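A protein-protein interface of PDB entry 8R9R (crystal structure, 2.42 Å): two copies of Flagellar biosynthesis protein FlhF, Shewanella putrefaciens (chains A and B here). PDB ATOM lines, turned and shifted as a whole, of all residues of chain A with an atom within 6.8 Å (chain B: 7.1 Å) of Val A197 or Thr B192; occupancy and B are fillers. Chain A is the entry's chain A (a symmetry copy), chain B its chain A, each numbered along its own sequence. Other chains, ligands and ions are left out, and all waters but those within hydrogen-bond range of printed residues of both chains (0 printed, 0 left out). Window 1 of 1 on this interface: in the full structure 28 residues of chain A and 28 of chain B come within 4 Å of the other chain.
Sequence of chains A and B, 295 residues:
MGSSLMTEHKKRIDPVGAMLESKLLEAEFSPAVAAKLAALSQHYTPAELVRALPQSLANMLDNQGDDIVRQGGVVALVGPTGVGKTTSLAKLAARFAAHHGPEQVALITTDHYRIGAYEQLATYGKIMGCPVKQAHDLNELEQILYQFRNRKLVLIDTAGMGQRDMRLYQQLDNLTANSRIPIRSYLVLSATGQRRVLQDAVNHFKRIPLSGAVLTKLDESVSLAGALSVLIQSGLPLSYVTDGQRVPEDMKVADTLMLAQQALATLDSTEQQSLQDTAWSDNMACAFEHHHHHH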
ATOM      1  N   PRO A  80      -1.814  -9.156  -1.807  1.00  0.00           N
ATOM      2  CA  PRO A  80      -2.204  -9.576  -0.463  1.00  0.00           C
ATOM      3  C   PRO A  80      -3.595  -9.050  -0.113  1.00  0.00           C
ATOM      4  O   PRO A  80      -4.247  -8.424  -0.938  1.00  0.00           O
ATOM      5  CB  PRO A  80      -1.080  -9.021   0.420  1.00  0.00           C
ATOM      6  CG  PRO A  80      -0.512  -7.849  -0.349  1.00  0.00           C
ATOM      7  CD  PRO A  80      -0.794  -8.093  -1.817  1.00  0.00           C
ATOM      8  N   GLN A 163       1.302 -12.768   1.851  1.00  0.00           N
ATOM      9  CA  GLN A 163       2.362 -13.042   0.895  1.00  0.00           C
ATOM     10  C   GLN A 163       3.169 -14.294   1.236  1.00  0.00           C
ATOM     11  O   GLN A 163       3.769 -14.881   0.343  1.00  0.00           O
ATOM     12  CB  GLN A 163       3.304 -11.825   0.722  1.00  0.00           C
ATOM     13  CG  GLN A 163       4.180 -11.473   1.930  1.00  0.00           C
ATOM     14  CD  GLN A 163       3.502 -10.583   2.948  1.00  0.00           C
ATOM     15  OE1 GLN A 163       2.303 -10.313   2.884  1.00  0.00           O
ATOM     16  NE2 GLN A 163       4.264 -10.089   3.912  1.00  0.00           N
ATOM     17  N   ARG A 164       3.172 -14.704   2.513  1.00  0.00           N
ATOM     18  CA  ARG A 164       3.865 -15.915   2.931  1.00  0.00           C
ATOM     19  C   ARG A 164       2.922 -17.088   3.203  1.00  0.00           C
ATOM     20  O   ARG A 164       3.303 -18.054   3.856  1.00  0.00           O
ATOM     21  CB  ARG A 164       4.719 -15.634   4.182  1.00  0.00           C
ATOM     22  CG  ARG A 164       5.765 -14.565   3.948  1.00  0.00           C
ATOM     23  CD  ARG A 164       6.672 -14.361   5.138  1.00  0.00           C
ATOM     24  NE  ARG A 164       5.926 -13.918   6.312  1.00  0.00           N
ATOM     25  CZ  ARG A 164       6.026 -12.713   6.868  1.00  0.00           C
ATOM     26  NH1 ARG A 164       6.731 -11.743   6.302  1.00  0.00           N
ATOM     27  NH2 ARG A 164       5.398 -12.475   8.019  1.00  0.00           N
ATOM     28  N   LEU A 189      -0.988  -3.444  -4.700  1.00  0.00           N
ATOM     29  CA  LEU A 189      -0.406  -3.135  -3.404  1.00  0.00           C
ATOM     30  C   LEU A 189      -0.970  -1.813  -2.899  1.00  0.00           C
ATOM     31  O   LEU A 189      -1.204  -0.892  -3.676  1.00  0.00           O
ATOM     32  CB  LEU A 189       1.106  -2.991  -3.502  1.00  0.00           C
ATOM     33  CG  LEU A 189       1.897  -4.202  -3.934  1.00  0.00           C
ATOM     34  CD1 LEU A 189       3.384  -3.821  -4.115  1.00  0.00           C
ATOM     35  CD2 LEU A 189       1.749  -5.330  -2.943  1.00  0.00           C
ATOM     36  N   THR A 192      -0.314   2.374   1.748  1.00  0.00           N
ATOM     37  CA  THR A 192      -0.215   2.486   3.195  1.00  0.00           C
ATOM     38  C   THR A 192       0.802   1.543   3.834  1.00  0.00           C
ATOM     39  O   THR A 192       1.182   1.746   4.983  1.00  0.00           O
ATOM     40  CB  THR A 192      -1.572   2.220   3.828  1.00  0.00           C
ATOM     41  OG1 THR A 192      -2.058   0.949   3.364  1.00  0.00           O
ATOM     42  CG2 THR A 192      -2.570   3.310   3.504  1.00  0.00           C
ATOM     43  N   GLY A 193       1.229   0.516   3.094  1.00  0.00           N
ATOM     44  CA  GLY A 193       2.081  -0.522   3.648  1.00  0.00           C
ATOM     45  C   GLY A 193       3.512  -0.082   3.952  1.00  0.00           C
ATOM     46  O   GLY A 193       4.094   0.736   3.234  1.00  0.00           O
ATOM     47  N   GLN A 194       4.090  -0.647   5.016  1.00  0.00           N
ATOM     48  CA  GLN A 194       5.507  -0.465   5.287  1.00  0.00           C
ATOM     49  C   GLN A 194       6.317  -0.891   4.070  1.00  0.00           C
ATOM     50  O   GLN A 194       5.942  -1.824   3.364  1.00  0.00           O
ATOM     51  CB  GLN A 194       5.945  -1.275   6.503  1.00  0.00           C
ATOM     52  CG  GLN A 194       5.382  -0.728   7.790  1.00  0.00           C
ATOM     53  CD  GLN A 194       5.569  -1.673   8.931  1.00  0.00           C
ATOM     54  OE1 GLN A 194       6.453  -2.532   8.928  1.00  0.00           O
ATOM     55  NE2 GLN A 194       4.738  -1.523   9.946  1.00  0.00           N
ATOM     56  N   ARG A 195       7.436  -0.204   3.843  1.00  0.00           N
ATOM     57  CA  ARG A 195       8.274  -0.459   2.685  1.00  0.00           C
ATOM     58  C   ARG A 195       8.679  -1.931   2.628  1.00  0.00           C
ATOM     59  O   ARG A 195       8.560  -2.577   1.587  1.00  0.00           O
ATOM     60  CB  ARG A 195       9.507   0.456   2.710  1.00  0.00           C
ATOM     61  CG  ARG A 195      10.184   0.557   1.363  1.00  0.00           C
ATOM     62  CD  ARG A 195      11.416   1.433   1.388  1.00  0.00           C
ATOM     63  NE  ARG A 195      12.452   0.900   2.269  1.00  0.00           N
ATOM     64  CZ  ARG A 195      12.885   1.500   3.370  1.00  0.00           C
ATOM     65  NH1 ARG A 195      12.364   2.647   3.781  1.00  0.00           N
ATOM     66  NH2 ARG A 195      13.855   0.931   4.082  1.00  0.00           N
ATOM     67  N   ARG A 196       9.115  -2.464   3.772  1.00  0.00           N
ATOM     68  CA  ARG A 196       9.628  -3.822   3.834  1.00  0.00           C
ATOM     69  C   ARG A 196       8.543  -4.873   3.601  1.00  0.00           C
ATOM     70  O   ARG A 196       8.810  -5.919   3.011  1.00  0.00           O
ATOM     71  CB  ARG A 196      10.328  -4.027   5.172  1.00  0.00           C
ATOM     72  CG  ARG A 196      11.538  -3.094   5.355  1.00  0.00           C
ATOM     73  CD  ARG A 196      12.172  -3.284   6.706  1.00  0.00           C
ATOM     74  NE  ARG A 196      12.627  -4.659   6.873  1.00  0.00           N
ATOM     75  CZ  ARG A 196      12.809  -5.255   8.043  1.00  0.00           C
ATOM     76  NH1 ARG A 196      12.553  -4.635   9.184  1.00  0.00           N
ATOM     77  NH2 ARG A 196      13.236  -6.514   8.068  1.00  0.00           N
ATOM     78  N   VAL A 197       7.317  -4.583   4.052  1.00  0.00           N
ATOM     79  CA  VAL A 197       6.169  -5.430   3.772  1.00  0.00           C
ATOM     80  C   VAL A 197       5.890  -5.466   2.271  1.00  0.00           C
ATOM     81  O   VAL A 197       5.726  -6.540   1.695  1.00  0.00           O
ATOM     82  CB  VAL A 197       4.923  -4.962   4.560  1.00  0.00           C
ATOM     83  CG1 VAL A 197       3.655  -5.651   4.055  1.00  0.00           C
ATOM     84  CG2 VAL A 197       5.108  -5.178   6.059  1.00  0.00           C
ATOM     85  N   LEU A 198       5.832  -4.284   1.648  1.00  0.00           N
ATOM     86  CA  LEU A 198       5.594  -4.197   0.218  1.00  0.00           C
ATOM     87  C   LEU A 198       6.653  -4.974  -0.558  1.00  0.00           C
ATOM     88  O   LEU A 198       6.324  -5.688  -1.498  1.00  0.00           O
ATOM     89  CB  LEU A 198       5.571  -2.744  -0.237  1.00  0.00           C
ATOM     90  CG  LEU A 198       4.472  -1.875   0.377  1.00  0.00           C
ATOM     91  CD1 LEU A 198       4.340  -0.566  -0.374  1.00  0.00           C
ATOM     92  CD2 LEU A 198       3.141  -2.584   0.409  1.00  0.00           C
ATOM     93  N   GLN A 199       7.917  -4.851  -0.138  1.00  0.00           N
ATOM     94  CA  GLN A 199       9.005  -5.566  -0.785  1.00  0.00           C
ATOM     95  C   GLN A 199       8.858  -7.071  -0.578  1.00  0.00           C
ATOM     96  O   GLN A 199       9.107  -7.852  -1.494  1.00  0.00           O
ATOM     97  CB  GLN A 199      10.373  -5.093  -0.251  1.00  0.00           C
ATOM     98  CG  GLN A 199      11.566  -5.643  -1.035  1.00  0.00           C
ATOM     99  CD  GLN A 199      11.509  -5.230  -2.496  1.00  0.00           C
ATOM    100  OE1 GLN A 199      11.668  -4.044  -2.844  1.00  0.00           O
ATOM    101  NE2 GLN A 199      11.270  -6.194  -3.389  1.00  0.00           N
ATOM    102  N   ASP A 200       8.474  -7.467   0.643  1.00  0.00           N
ATOM    103  CA  ASP A 200       8.265  -8.869   0.969  1.00  0.00           C
ATOM    104  C   ASP A 200       7.159  -9.433   0.077  1.00  0.00           C
ATOM    105  O   ASP A 200       7.332 -10.488  -0.527  1.00  0.00           O
ATOM    106  CB  ASP A 200       7.937  -9.034   2.469  1.00  0.00           C
ATOM    107  CG  ASP A 200       7.941 -10.466   2.974  1.00  0.00           C
ATOM    108  OD1 ASP A 200       8.906 -11.197   2.672  1.00  0.00           O
ATOM    109  OD2 ASP A 200       6.985 -10.850   3.685  1.00  0.00           O
ATOM    110  N   ALA A 201       6.048  -8.690  -0.033  1.00  0.00           N
ATOM    111  CA  ALA A 201       4.966  -9.037  -0.941  1.00  0.00           C
ATOM    112  C   ALA A 201       5.476  -9.217  -2.365  1.00  0.00           C
ATOM    113  O   ALA A 201       5.201 -10.238  -2.994  1.00  0.00           O
ATOM    114  CB  ALA A 201       3.865  -7.986  -0.912  1.00  0.00           C
ATOM    115  N   VAL A 202       6.223  -8.224  -2.861  1.00  0.00           N
ATOM    116  CA  VAL A 202       6.747  -8.267  -4.217  1.00  0.00           C
ATOM    117  C   VAL A 202       7.530  -9.558  -4.440  1.00  0.00           C
ATOM    118  O   VAL A 202       7.268 -10.288  -5.394  1.00  0.00           O
ATOM    119  CB  VAL A 202       7.625  -7.038  -4.549  1.00  0.00           C
ATOM    120  CG1 VAL A 202       8.413  -7.256  -5.834  1.00  0.00           C
ATOM    121  CG2 VAL A 202       6.793  -5.767  -4.637  1.00  0.00           C
ATOM    122  N   ASN A 203       8.489  -9.831  -3.548  1.00  0.00           N
ATOM    123  CA  ASN A 203       9.358 -10.990  -3.682  1.00  0.00           C
ATOM    124  C   ASN A 203       8.579 -12.304  -3.799  1.00  0.00           C
ATOM    125  O   ASN A 203       8.915 -13.154  -4.620  1.00  0.00           O
ATOM    126  CB  ASN A 203      10.319 -11.056  -2.508  1.00  0.00           C
ATOM    127  CG  ASN A 203      11.264  -9.866  -2.404  1.00  0.00           C
ATOM    128  OD1 ASN A 203      11.397  -9.031  -3.321  1.00  0.00           O
ATOM    129  ND2 ASN A 203      11.962  -9.774  -1.273  1.00  0.00           N
ATOM    130  N   VAL A 230       9.943   0.766  -3.764  1.00  0.00           N
ATOM    131  CA  VAL A 230       9.844  -0.677  -3.928  1.00  0.00           C
ATOM    132  C   VAL A 230       9.599  -1.066  -5.389  1.00  0.00           C
ATOM    133  O   VAL A 230      10.199  -2.021  -5.882  1.00  0.00           O
ATOM    134  CB  VAL A 230       8.758  -1.270  -2.981  1.00  0.00           C
ATOM    135  CG1 VAL A 230       8.450  -2.721  -3.318  1.00  0.00           C
ATOM    136  CG2 VAL A 230       9.164  -1.144  -1.514  1.00  0.00           C
ATOM    137  N   LEU B 189      -6.613  -2.098  13.265  1.00  0.00           N
ATOM    138  CA  LEU B 189      -5.513  -1.628  12.438  1.00  0.00           C
ATOM    139  C   LEU B 189      -4.658  -2.816  12.013  1.00  0.00           C
ATOM    140  O   LEU B 189      -4.462  -3.754  12.780  1.00  0.00           O
ATOM    141  CB  LEU B 189      -4.623  -0.661  13.205  1.00  0.00           C
ATOM    142  CG  LEU B 189      -5.243   0.629  13.684  1.00  0.00           C
ATOM    143  CD1 LEU B 189      -4.232   1.403  14.560  1.00  0.00           C
ATOM    144  CD2 LEU B 189      -5.705   1.475  12.523  1.00  0.00           C
ATOM    145  N   SER B 190      -4.143  -2.753  10.787  1.00  0.00           N
ATOM    146  CA  SER B 190      -3.268  -3.778  10.257  1.00  0.00           C
ATOM    147  C   SER B 190      -1.819  -3.457  10.611  1.00  0.00           C
ATOM    148  O   SER B 190      -1.375  -2.319  10.460  1.00  0.00           O
ATOM    149  CB  SER B 190      -3.443  -3.895   8.745  1.00  0.00           C
ATOM    150  OG  SER B 190      -2.517  -4.825   8.209  1.00  0.00           O
ATOM    151  N   ALA B 191      -1.089  -4.483  11.059  1.00  0.00           N
ATOM    152  CA  ALA B 191       0.301  -4.341  11.455  1.00  0.00           C
ATOM    153  C   ALA B 191       1.246  -4.146  10.270  1.00  0.00           C
ATOM    154  O   ALA B 191       2.445  -3.953  10.470  1.00  0.00           O
ATOM    155  CB  ALA B 191       0.716  -5.561  12.249  1.00  0.00           C
ATOM    156  N   THR B 192       0.705  -4.218   9.043  1.00  0.00           N
ATOM    157  CA  THR B 192       1.463  -3.934   7.834  1.00  0.00           C
ATOM    158  C   THR B 192       1.621  -2.447   7.522  1.00  0.00           C
ATOM    159  O   THR B 192       2.470  -2.082   6.715  1.00  0.00           O
ATOM    160  CB  THR B 192       0.801  -4.601   6.639  1.00  0.00           C
ATOM    161  OG1 THR B 192      -0.576  -4.193   6.584  1.00  0.00           O
ATOM    162  CG2 THR B 192       0.894  -6.110   6.711  1.00  0.00           C
ATOM    163  N   GLY B 193       0.800  -1.602   8.152  1.00  0.00           N
ATOM    164  CA  GLY B 193       0.763  -0.188   7.825  1.00  0.00           C
ATOM    165  C   GLY B 193       1.995   0.604   8.262  1.00  0.00           C
ATOM    166  O   GLY B 193       2.590   0.330   9.308  1.00  0.00           O
ATOM    167  N   GLN B 194       2.366   1.608   7.462  1.00  0.00           N
ATOM    168  CA  GLN B 194       3.391   2.555   7.872  1.00  0.00           C
ATOM    169  C   GLN B 194       3.005   3.178   9.207  1.00  0.00           C
ATOM    170  O   GLN B 194       1.826   3.392   9.481  1.00  0.00           O
ATOM    171  CB  GLN B 194       3.574   3.653   6.829  1.00  0.00           C
ATOM    172  CG  GLN B 194       4.213   3.141   5.563  1.00  0.00           C
ATOM    173  CD  GLN B 194       4.130   4.134   4.451  1.00  0.00           C
ATOM    174  OE1 GLN B 194       3.999   5.342   4.663  1.00  0.00           O
ATOM    175  NE2 GLN B 194       4.220   3.641   3.230  1.00  0.00           N
ATOM    176  N   ARG B 195       4.014   3.474  10.026  1.00  0.00           N
ATOM    177  CA  ARG B 195       3.791   4.014  11.355  1.00  0.00           C
ATOM    178  C   ARG B 195       2.934   5.277  11.287  1.00  0.00           C
ATOM    179  O   ARG B 195       1.957   5.417  12.023  1.00  0.00           O
ATOM    180  CB  ARG B 195       5.134   4.290  12.048  1.00  0.00           C
ATOM    181  CG  ARG B 195       4.997   4.440  13.545  1.00  0.00           C
ATOM    182  CD  ARG B 195       6.311   4.741  14.229  1.00  0.00           C
ATOM    183  NE  ARG B 195       6.877   6.015  13.794  1.00  0.00           N
ATOM    184  CZ  ARG B 195       8.019   6.144  13.132  1.00  0.00           C
ATOM    185  NH1 ARG B 195       8.732   5.086  12.774  1.00  0.00           N
ATOM    186  NH2 ARG B 195       8.450   7.361  12.809  1.00  0.00           N
ATOM    187  N   LEU B 198      -0.736   4.616  10.453  1.00  0.00           N
ATOM    188  CA  LEU B 198      -1.421   4.102  11.625  1.00  0.00           C
ATOM    189  C   LEU B 198      -1.731   5.225  12.610  1.00  0.00           C
ATOM    190  O   LEU B 198      -2.829   5.280  13.153  1.00  0.00           O
ATOM    191  CB  LEU B 198      -0.589   3.023  12.306  1.00  0.00           C
ATOM    192  CG  LEU B 198      -0.305   1.778  11.465  1.00  0.00           C
ATOM    193  CD1 LEU B 198       0.237   0.658  12.330  1.00  0.00           C
ATOM    194  CD2 LEU B 198      -1.529   1.304  10.722  1.00  0.00           C
ATOM    195  N   LEU B 215      -5.151  -5.694  16.526  1.00  0.00           N
ATOM    196  CA  LEU B 215      -4.024  -5.622  15.616  1.00  0.00           C
ATOM    197  C   LEU B 215      -4.071  -6.837  14.695  1.00  0.00           C
ATOM    198  O   LEU B 215      -3.914  -7.965  15.149  1.00  0.00           O
ATOM    199  CB  LEU B 215      -2.727  -5.557  16.427  1.00  0.00           C
ATOM    200  CG  LEU B 215      -1.550  -4.933  15.719  1.00  0.00           C
ATOM    201  CD1 LEU B 215      -1.852  -3.491  15.336  1.00  0.00           C
ATOM    202  CD2 LEU B 215      -0.294  -5.006  16.586  1.00  0.00           C
ATOM    203  N   THR B 216      -4.310  -6.589  13.401  1.00  0.00           N
ATOM    204  CA  THR B 216      -4.482  -7.661  12.438  1.00  0.00           C
ATOM    205  C   THR B 216      -3.260  -7.892  11.555  1.00  0.00           C
ATOM    206  O   THR B 216      -2.386  -7.037  11.451  1.00  0.00           O
ATOM    207  CB  THR B 216      -5.707  -7.377  11.569  1.00  0.00           C
ATOM    208  OG1 THR B 216      -5.474  -6.171  10.835  1.00  0.00           O
ATOM    209  CG2 THR B 216      -6.994  -7.267  12.389  1.00  0.00           C
ATOM    210  N   LYS B 217      -3.226  -9.079  10.942  1.00  0.00           N
ATOM    211  CA  LYS B 217      -2.293  -9.423   9.883  1.00  0.00           C
ATOM    212  C   LYS B 217      -0.850  -9.468  10.369  1.00  0.00           C
ATOM    213  O   LYS B 217       0.060  -9.036   9.671  1.00  0.00           O
ATOM    214  CB  LYS B 217      -2.435  -8.462   8.704  1.00  0.00           C
ATOM    215  CG  LYS B 217      -3.879  -8.252   8.286  1.00  0.00           C
ATOM    216  CD  LYS B 217      -4.037  -7.636   6.929  1.00  0.00           C
ATOM    217  CE  LYS B 217      -5.497  -7.429   6.609  1.00  0.00           C
ATOM    218  NZ  LYS B 217      -5.684  -6.951   5.228  1.00  0.00           N
ATOM    219  N   LEU B 218      -0.646 -10.055  11.552  1.00  0.00           N
ATOM    220  CA  LEU B 218       0.695 -10.305  12.054  1.00  0.00           C
ATOM    221  C   LEU B 218       1.433 -11.305  11.164  1.00  0.00           C
ATOM    222  O   LEU B 218       2.653 -11.245  11.037  1.00  0.00           O
ATOM    223  CB  LEU B 218       0.632 -10.777  13.508  1.00  0.00           C
ATOM    224  CG  LEU B 218       0.541  -9.659  14.556  1.00  0.00           C
ATOM    225  CD1 LEU B 218      -0.774  -8.900  14.457  1.00  0.00           C
ATOM    226  CD2 LEU B 218       0.700 -10.213  15.943  1.00  0.00           C
ATOM    227  N   ASP B 219       0.677 -12.196  10.512  1.00  0.00           N
ATOM    228  CA  ASP B 219       1.237 -13.136   9.550  1.00  0.00           C
ATOM    229  C   ASP B 219       1.717 -12.500   8.243  1.00  0.00           C
ATOM    230  O   ASP B 219       2.431 -13.148   7.482  1.00  0.00           O
ATOM    231  CB  ASP B 219       0.200 -14.222   9.248  1.00  0.00           C
ATOM    232  CG  ASP B 219      -1.062 -13.702   8.589  1.00  0.00           C
ATOM    233  OD1 ASP B 219      -1.699 -12.786   9.161  1.00  0.00           O
ATOM    234  OD2 ASP B 219      -1.413 -14.207   7.498  1.00  0.00           O
ATOM    235  N   GLU B 220       1.312 -11.249   7.977  1.00  0.00           N
ATOM    236  CA  GLU B 220       1.805 -10.477   6.841  1.00  0.00           C
ATOM    237  C   GLU B 220       2.879  -9.448   7.202  1.00  0.00           C
ATOM    238  O   GLU B 220       3.472  -8.832   6.317  1.00  0.00           O
ATOM    239  CB  GLU B 220       0.649  -9.711   6.174  1.00  0.00           C
ATOM    240  CG  GLU B 220      -0.212 -10.549   5.251  1.00  0.00           C
ATOM    241  CD  GLU B 220      -1.338  -9.798   4.559  1.00  0.00           C
ATOM    242  OE1 GLU B 220      -1.152  -8.599   4.263  1.00  0.00           O
ATOM    243  OE2 GLU B 220      -2.387 -10.419   4.268  1.00  0.00           O
ATOM    244  N   SER B 221       3.102  -9.243   8.504  1.00  0.00           N
ATOM    245  CA  SER B 221       3.982  -8.191   8.983  1.00  0.00           C
ATOM    246  C   SER B 221       5.440  -8.636   8.987  1.00  0.00           C
ATOM    247  O   SER B 221       5.732  -9.797   9.243  1.00  0.00           O
ATOM    248  CB  SER B 221       3.568  -7.753  10.382  1.00  0.00           C
ATOM    249  OG  SER B 221       2.264  -7.190  10.355  1.00  0.00           O
ATOM    250  N   VAL B 222       6.338  -7.698   8.681  1.00  0.00           N
ATOM    251  CA  VAL B 222       7.764  -7.894   8.881  1.00  0.00           C
ATOM    252  C   VAL B 222       8.109  -7.561  10.328  1.00  0.00           C
ATOM    253  O   VAL B 222       8.780  -8.338  10.992  1.00  0.00           O
ATOM    254  CB  VAL B 222       8.590  -7.051   7.889  1.00  0.00           C
ATOM    255  CG1 VAL B 222      10.041  -6.957   8.326  1.00  0.00           C
ATOM    256  CG2 VAL B 222       8.491  -7.605   6.474  1.00  0.00           C
ATOM    257  N   SER B 223       7.636  -6.402  10.804  1.00  0.00           N
ATOM    258  CA  SER B 223       7.951  -5.919  12.139  1.00  0.00           C
ATOM    259  C   SER B 223       6.757  -5.297  12.859  1.00  0.00           C
ATOM    260  O   SER B 223       5.981  -4.556  12.268  1.00  0.00           O
ATOM    261  CB  SER B 223       9.064  -4.881  12.071  1.00  0.00           C
ATOM    262  OG  SER B 223       9.278  -4.290  13.344  1.00  0.00           O
ATOM    263  N   ALA B 227       3.900  -0.439  14.816  1.00  0.00           N
ATOM    264  CA  ALA B 227       2.512  -0.629  15.193  1.00  0.00           C
ATOM    265  C   ALA B 227       2.346  -0.557  16.707  1.00  0.00           C
ATOM    266  O   ALA B 227       1.484   0.161  17.211  1.00  0.00           O
ATOM    267  CB  ALA B 227       1.994  -1.963  14.662  1.00  0.00           C
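Thr A192 touches Gly B193, and with the chains exchanged Gly A193 touches Thr B192. Thr A192 touches Gln B194, and with the chains exchanged Gln A194 touches Thr B192. Gly A193 touches Gln B194, and with the chains exchanged Gln A194 touches Gly B193. Gln B194 touches its own counterpart, Gln A194. Of the 17 pairs that touch across the chains among the printed residues, 7 have their exchanged pair printed and touching as well.
OG1 of Thr B192 sits at hydrogen-bond distance from OG of Ser B190, at 2.6 Å. O of Thr B216 sits at hydrogen-bond distance from N of Ala B191 (2.9 Å). The side-chain hydroxyl (OG) of Ser B221 lies close to the backbone carbonyl oxygen (O) of Ala B191, 3.2 Å away. The backbone carbonyl oxygen (O) of Lys B217 sits at hydrogen-bond distance from the side-chain hydroxyl (OG) of Ser B221. The side-chain amide nitrogen (NE2) of Gln A163 lies within hydrogen-bond range of the side-chain carboxylate (OD2) of Asp A200, at 2.8 Å. The side-chain carboxylate (OD2) of Asp A200 is in salt-bridge range of the guanidinium group (NH1) of Arg A164.
Glu B220 touches Pro A80. Gly B193 touches Thr A192 (CA to O, 3.5 Å). Gly A193 touches Thr B192. N of Gln A194 touches N of Gln B194, 3.7 Å away. O of Ser B223 touches OE1 of Gln A194, at 3.9 Å. Arg A196 touches Val B222. Thr B192 touches Val A197. CG1 of Val A197 touches O of Glu B220 (3.9 Å). CG2 of Val A197 touches N of Val B222, at 3.8 Å.
Val A197 touches three residues of chain B. Of the printed residues of chain B, Gln A194 touches Ala B191 (3.4 Å), Thr B192 (2.8 Å), Gly B193 (2.9 Å), Gln B194 (3.7 Å) and Ser B223 (3.9 Å). Printed residues of chain A within 4 Å of Glu B220: Pro A80 (3.9 Å), Gln A163 (2.8 Å) and Val A197 (3.9 Å). Arg B195 touches none of the printed residues of chain A. The nearest residue of chain B that does not touch Val A197 is Ser B221 (4.3 Å). The nearest printed residue of chain B that does not touch Pro A80 is Lys B217 (6.1 Å).
The side-chain amide nitrogen of Gln A194 is in hydrogen-bond range of the backbone carbonyl oxygen of Ala B191 (3.4 Å). The backbone carbonyl oxygen of Thr B192 lies within hydrogen-bond range of the backbone NH of Gln A194 (2.8 Å). The backbone carbonyl oxygen (O) of Gly B193 lies within hydrogen-bond range of the side-chain amide nitrogen (NE2) of Gln A194 (2.9 Å). N of Gln B194 lies within hydrogen-bond range of O of Thr A192 (2.8 Å). NE2 of Gln B194 is in hydrogen-bond range of O of Gly A193, 2.9 Å away. The backbone carbonyl oxygen (O) of Asp B219 is in hydrogen-bond range of the guanidinium group (NH2) of Arg A164, 3.1 Å away. The backbone carbonyl oxygen (O) of Glu B220 is in hydrogen-bond range of the side-chain amide nitrogen (NE2) of Gln A163, at 2.8 Å. The guanidinium group (NH2) of Arg A164 is in hydrogen-bond range of the backbone carbonyl oxygen (O) of Ser B221, at 3.0 Å.
Of the 18 printed residues of chain B, 9 touch a printed residue of chain A. Among the printed residues, no Asp or Glu carboxylate lies within 4 Å of a Lys or Arg side-chain nitrogen of the other chain.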
